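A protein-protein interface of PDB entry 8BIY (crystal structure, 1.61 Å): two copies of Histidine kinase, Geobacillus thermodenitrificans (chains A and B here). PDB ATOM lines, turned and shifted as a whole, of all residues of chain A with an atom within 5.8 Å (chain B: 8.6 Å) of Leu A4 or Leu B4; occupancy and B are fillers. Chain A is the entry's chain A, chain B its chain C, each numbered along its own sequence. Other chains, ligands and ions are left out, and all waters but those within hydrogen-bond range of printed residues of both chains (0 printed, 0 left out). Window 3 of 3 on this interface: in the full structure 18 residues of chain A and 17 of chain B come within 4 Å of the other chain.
Hydrophobic or aromatic side chains of chain A that line the printed part of chain B: Ile A8.
The guanidinium group (NH1) of Arg B11 lies close to the side-chain amide oxygen (OE1) of Gln A7 (3.3 Å).
Leu A4 touches its own counterpart, Leu B4. Gln A7 touches Leu B4, but with the chains exchanged Leu A4 does not touch Gln B7 (4.6 Å). Gln A7 touches Ile B8, and with the chains exchanged Ile A8 touches Gln B7. 6 positions are printed for both chains.
Among the printed residues, merely in contact across the chains: Thr A3 with Leu B4, Leu A4 with Leu B4, Gln A7 with Leu B4, Gln A7 with Ile B8 and Ile A8 with Gln B7.
OG1 of Thr A3 sits close to N of Lys A5, 3.3 Å away. The side-chain hydroxyl of Thr A3 sits at hydrogen-bond distance from the backbone NH of Glu A6 (2.9 Å).
Of the printed residues of chain B, Leu A4 touches Leu B4 (3.8 Å). No residue of chain B comes within 4 Å of Lys A5. Leu B4 touches just these residues of chain A: Thr A3 (3.5 Å), Leu A4 (3.8 Å) and Gln A7 (3.8 Å). Lys B5 touches none of the printed residues of chain A. Printed residues of chain A within 4 Å of Gln B7: Ile A8. Gly B9 touches none of the printed residues of chain A. Of the printed residues of chain A, Arg B11 touches Gln A7 (3.1 Å). The nearest printed residue of chain A that does not touch Leu B4 is Lys A5 (6.2 Å). The nearest printed residue of chain A that does not touch Arg B11 is Ile A8 (6.3 Å).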
ATOM      1  N   THR A   3     -33.895  25.458 -20.236  1.00  0.00           N
ATOM      2  CA  THR A   3     -35.103  24.931 -20.866  1.00  0.00           C
ATOM      3  C   THR A   3     -34.766  23.998 -22.033  1.00  0.00           C
ATOM      4  O   THR A   3     -33.780  24.211 -22.744  1.00  0.00           O
ATOM      5  CB  THR A   3     -36.017  26.071 -21.360  1.00  0.00           C
ATOM      6  OG1 THR A   3     -36.001  26.125 -22.791  1.00  0.00           O
ATOM      7  CG2 THR A   3     -35.555  27.405 -20.792  1.00  0.00           C
ATOM      8  N   LEU A   4     -35.591  22.960 -22.215  1.00  0.00           N
ATOM      9  CA  LEU A   4     -35.331  21.978 -23.265  1.00  0.00           C
ATOM     10  C   LEU A   4     -35.408  22.611 -24.648  1.00  0.00           C
ATOM     11  O   LEU A   4     -34.630  22.257 -25.543  1.00  0.00           O
ATOM     12  CB  LEU A   4     -36.311  20.809 -23.154  1.00  0.00           C
ATOM     13  N   LYS A   5     -36.335  23.552 -24.844  1.00  0.00           N
ATOM     14  CA  LYS A   5     -36.406  24.253 -26.121  1.00  0.00           C
ATOM     15  C   LYS A   5     -35.146  25.071 -26.369  1.00  0.00           C
ATOM     16  O   LYS A   5     -34.640  25.111 -27.497  1.00  0.00           O
ATOM     17  CB  LYS A   5     -37.644  25.152 -26.168  1.00  0.00           C
ATOM     18  N   GLU A   6     -34.625  25.733 -25.331  1.00  0.00           N
ATOM     19  CA  GLU A   6     -33.413  26.527 -25.503  1.00  0.00           C
ATOM     20  C   GLU A   6     -32.215  25.650 -25.832  1.00  0.00           C
ATOM     21  O   GLU A   6     -31.321  26.081 -26.571  1.00  0.00           O
ATOM     22  CB  GLU A   6     -33.116  27.351 -24.250  1.00  0.00           C
ATOM     23  CG  GLU A   6     -33.823  28.692 -24.181  1.00  0.00           C
ATOM     24  CD  GLU A   6     -33.245  29.597 -23.103  1.00  0.00           C
ATOM     25  OE1 GLU A   6     -33.134  29.155 -21.937  1.00  0.00           O
ATOM     26  OE2 GLU A   6     -32.895  30.752 -23.424  1.00  0.00           O
ATOM     27  N   GLN A   7     -32.176  24.429 -25.291  1.00  0.00           N
ATOM     28  CA  GLN A   7     -31.076  23.518 -25.587  1.00  0.00           C
ATOM     29  C   GLN A   7     -31.192  22.952 -26.996  1.00  0.00           C
ATOM     30  O   GLN A   7     -30.174  22.749 -27.670  1.00  0.00           O
ATOM     31  CB  GLN A   7     -31.022  22.389 -24.555  1.00  0.00           C
ATOM     32  CG  GLN A   7     -30.261  22.730 -23.271  1.00  0.00           C
ATOM     33  CD  GLN A   7     -28.859  23.263 -23.537  1.00  0.00           C
ATOM     34  OE1 GLN A   7     -28.102  22.685 -24.312  1.00  0.00           O
ATOM     35  NE2 GLN A   7     -28.508  24.365 -22.882  1.00  0.00           N
ATOM     36  N   ILE A   8     -32.419  22.693 -27.466  1.00  0.00           N
ATOM     37  CA  ILE A   8     -32.589  22.262 -28.851  1.00  0.00           C
ATOM     38  C   ILE A   8     -32.142  23.366 -29.797  1.00  0.00           C
ATOM     39  O   ILE A   8     -31.571  23.100 -30.863  1.00  0.00           O
ATOM     40  CB  ILE A   8     -34.046  21.851 -29.139  1.00  0.00           C
ATOM     41  CG1 ILE A   8     -34.494  20.706 -28.248  1.00  0.00           C
ATOM     42  CG2 ILE A   8     -34.168  21.342 -30.562  1.00  0.00           C
ATOM     43  CD1 ILE A   8     -36.002  20.609 -28.179  1.00  0.00           C
ATOM     44  N   GLY A   9     -32.407  24.624 -29.432  1.00  0.00           N
ATOM     45  CA  GLY A   9     -31.925  25.739 -30.232  1.00  0.00           C
ATOM     46  C   GLY A   9     -30.413  25.845 -30.235  1.00  0.00           C
ATOM     47  O   GLY A   9     -29.808  26.216 -31.247  1.00  0.00           O
ATOM     48  N   LEU B   4     -33.249  17.483 -20.237  1.00  0.00           N
ATOM     49  CA  LEU B   4     -32.288  18.545 -20.513  1.00  0.00           C
ATOM     50  C   LEU B   4     -30.881  17.980 -20.649  1.00  0.00           C
ATOM     51  O   LEU B   4     -30.145  18.327 -21.574  1.00  0.00           O
ATOM     52  CB  LEU B   4     -32.319  19.604 -19.414  1.00  0.00           C
ATOM     53  CG  LEU B   4     -31.555  20.888 -19.739  1.00  0.00           C
ATOM     54  CD1 LEU B   4     -32.499  21.966 -20.265  1.00  0.00           C
ATOM     55  CD2 LEU B   4     -30.776  21.380 -18.527  1.00  0.00           C
ATOM     56  N   LYS B   5     -30.513  17.117 -19.698  1.00  0.00           N
ATOM     57  CA  LYS B   5     -29.248  16.397 -19.793  1.00  0.00           C
ATOM     58  C   LYS B   5     -29.167  15.613 -21.094  1.00  0.00           C
ATOM     59  O   LYS B   5     -28.098  15.530 -21.712  1.00  0.00           O
ATOM     60  CB  LYS B   5     -29.096  15.458 -18.597  1.00  0.00           C
ATOM     61  CG  LYS B   5     -27.875  15.717 -17.740  1.00  0.00           C
ATOM     62  CD  LYS B   5     -28.055  15.147 -16.339  1.00  0.00           C
ATOM     63  CE  LYS B   5     -27.743  13.662 -16.293  1.00  0.00           C
ATOM     64  NZ  LYS B   5     -27.754  13.136 -14.897  1.00  0.00           N
ATOM     65  N   GLU B   6     -30.290  15.037 -21.527  1.00  0.00           N
ATOM     66  CA  GLU B   6     -30.307  14.289 -22.778  1.00  0.00           C
ATOM     67  C   GLU B   6     -30.057  15.201 -23.973  1.00  0.00           C
ATOM     68  O   GLU B   6     -29.360  14.812 -24.917  1.00  0.00           O
ATOM     69  CB  GLU B   6     -31.639  13.554 -22.931  1.00  0.00           C
ATOM     70  N   GLN B   7     -30.613  16.419 -23.954  1.00  0.00           N
ATOM     71  CA  GLN B   7     -30.411  17.334 -25.077  1.00  0.00           C
ATOM     72  C   GLN B   7     -29.011  17.941 -25.084  1.00  0.00           C
ATOM     73  O   GLN B   7     -28.485  18.252 -26.160  1.00  0.00           O
ATOM     74  CB  GLN B   7     -31.472  18.435 -25.075  1.00  0.00           C
ATOM     75  CG  GLN B   7     -32.786  18.045 -25.751  1.00  0.00           C
ATOM     76  CD  GLN B   7     -32.586  17.467 -27.146  1.00  0.00           C
ATOM     77  OE1 GLN B   7     -31.999  18.108 -28.025  1.00  0.00           O
ATOM     78  NE2 GLN B   7     -33.077  16.251 -27.357  1.00  0.00           N
ATOM     79  N   ILE B   8     -28.397  18.143 -23.916  1.00  0.00           N
ATOM     80  CA  ILE B   8     -27.001  18.566 -23.916  1.00  0.00           C
ATOM     81  C   ILE B   8     -26.126  17.441 -24.449  1.00  0.00           C
ATOM     82  O   ILE B   8     -25.149  17.683 -25.168  1.00  0.00           O
ATOM     83  CB  ILE B   8     -26.552  19.021 -22.515  1.00  0.00           C
ATOM     84  CG1 ILE B   8     -27.242  20.323 -22.119  1.00  0.00           C
ATOM     85  CG2 ILE B   8     -25.073  19.337 -22.522  1.00  0.00           C
ATOM     86  CD1 ILE B   8     -27.805  20.305 -20.723  1.00  0.00           C
ATOM     87  N   GLY B   9     -26.473  16.192 -24.130  1.00  0.00           N
ATOM     88  CA  GLY B   9     -25.781  15.071 -24.736  1.00  0.00           C
ATOM     89  C   GLY B   9     -25.951  15.043 -26.243  1.00  0.00           C
ATOM     90  O   GLY B   9     -25.023  14.699 -26.978  1.00  0.00           O
ATOM     91  N   MET B  10     -27.140  15.420 -26.724  1.00  0.00           N
ATOM     92  CA  MET B  10     -27.375  15.476 -28.161  1.00  0.00           C
ATOM     93  C   MET B  10     -26.603  16.622 -28.803  1.00  0.00           C
ATOM     94  O   MET B  10     -26.134  16.486 -29.940  1.00  0.00           O
ATOM     95  CB  MET B  10     -28.873  15.603 -28.455  1.00  0.00           C
ATOM     96  CG  MET B  10     -29.700  14.389 -28.076  1.00  0.00           C
ATOM     97  SD  MET B  10     -29.061  12.879 -28.808  1.00  0.00           S
ATOM     98  CE  MET B  10     -29.177  13.251 -30.557  1.00  0.00           C
ATOM     99  N   ARG B  11     -26.476  17.762 -28.103  1.00  0.00           N
ATOM    100  CA  ARG B  11     -25.558  18.814 -28.538  1.00  0.00           C
ATOM    101  C   ARG B  11     -24.159  18.255 -28.752  1.00  0.00           C
ATOM    102  O   ARG B  11     -23.560  18.439 -29.818  1.00  0.00           O
ATOM    103  CB  ARG B  11     -25.483  19.940 -27.507  1.00  0.00           C
ATOM    104  CG  ARG B  11     -26.373  21.125 -27.736  1.00  0.00           C
ATOM    105  CD  ARG B  11     -26.134  22.149 -26.637  1.00  0.00           C
ATOM    106  NE  ARG B  11     -24.987  23.008 -26.915  1.00  0.00           N
ATOM    107  CZ  ARG B  11     -24.637  24.041 -26.159  1.00  0.00           C
ATOM    108  NH1 ARG B  11     -25.246  24.291 -25.008  1.00  0.00           N
ATOM    109  NH2 ARG B  11     -23.657  24.842 -26.563  1.00  0.00           N
ATOM    110  N   ILE B 102     -21.126  16.013 -20.005  1.00  0.00           N
ATOM    111  CA  ILE B 102     -21.722  14.983 -20.841  1.00  0.00           C
ATOM    112  C   ILE B 102     -21.024  15.058 -22.189  1.00  0.00           C
ATOM    113  O   ILE B 102     -20.728  16.153 -22.686  1.00  0.00           O
ATOM    114  CB  ILE B 102     -23.249  15.154 -20.976  1.00  0.00           C
ATOM    115  CG1 ILE B 102     -23.858  14.064 -21.856  1.00  0.00           C
ATOM    116  CG2 ILE B 102     -23.572  16.486 -21.549  1.00  0.00           C
ATOM    117  CD1 ILE B 102     -25.184  13.559 -21.338  1.00  0.00           C
ATOM    118  N   LEU B 125     -21.909  20.378 -17.612  1.00  0.00           N
ATOM    119  CA  LEU B 125     -23.316  20.398 -17.228  1.00  0.00           C
ATOM    120  C   LEU B 125     -23.575  21.677 -16.439  1.00  0.00           C
ATOM    121  O   LEU B 125     -23.396  21.741 -15.222  1.00  0.00           O
ATOM    122  CB  LEU B 125     -23.678  19.139 -16.450  1.00  0.00           C
ATOM    123  CG  LEU B 125     -23.739  17.913 -17.363  1.00  0.00           C
ATOM    124  CD1 LEU B 125     -23.591  16.609 -16.586  1.00  0.00           C
ATOM    125  CD2 LEU B 125     -25.028  17.913 -18.171  1.00  0.00           C
ATOM    126  N   GLU B 126     -23.980  22.716 -17.165  1.00  0.00           N
ATOM    127  CA  GLU B 126     -24.229  24.043 -16.623  1.00  0.00           C
ATOM    128  C   GLU B 126     -25.156  24.761 -17.593  1.00  0.00           C
ATOM    129  O   GLU B 126     -25.135  24.495 -18.798  1.00  0.00           O
ATOM    130  CB  GLU B 126     -22.929  24.844 -16.428  1.00  0.00           C
ATOM    131  CG  GLU B 126     -22.248  25.305 -17.728  1.00  0.00           C
ATOM    132  CD  GLU B 126     -20.921  26.022 -17.487  1.00  0.00           C
ATOM    133  OE1 GLU B 126     -20.595  26.304 -16.315  1.00  0.00           O
ATOM    134  OE2 GLU B 126     -20.214  26.338 -18.472  1.00  0.00           O
ATOM    135  N   ASP B 127     -25.978  25.657 -17.062  1.00  0.00           N
ATOM    136  CA  ASP B 127     -26.874  26.436 -17.909  1.00  0.00           C
ATOM    137  C   ASP B 127     -26.068  27.328 -18.854  1.00  0.00           C
ATOM    138  O   ASP B 127     -26.585  27.815 -19.862  1.00  0.00           O
ATOM    139  CB  ASP B 127     -27.827  27.276 -17.057  1.00  0.00           C
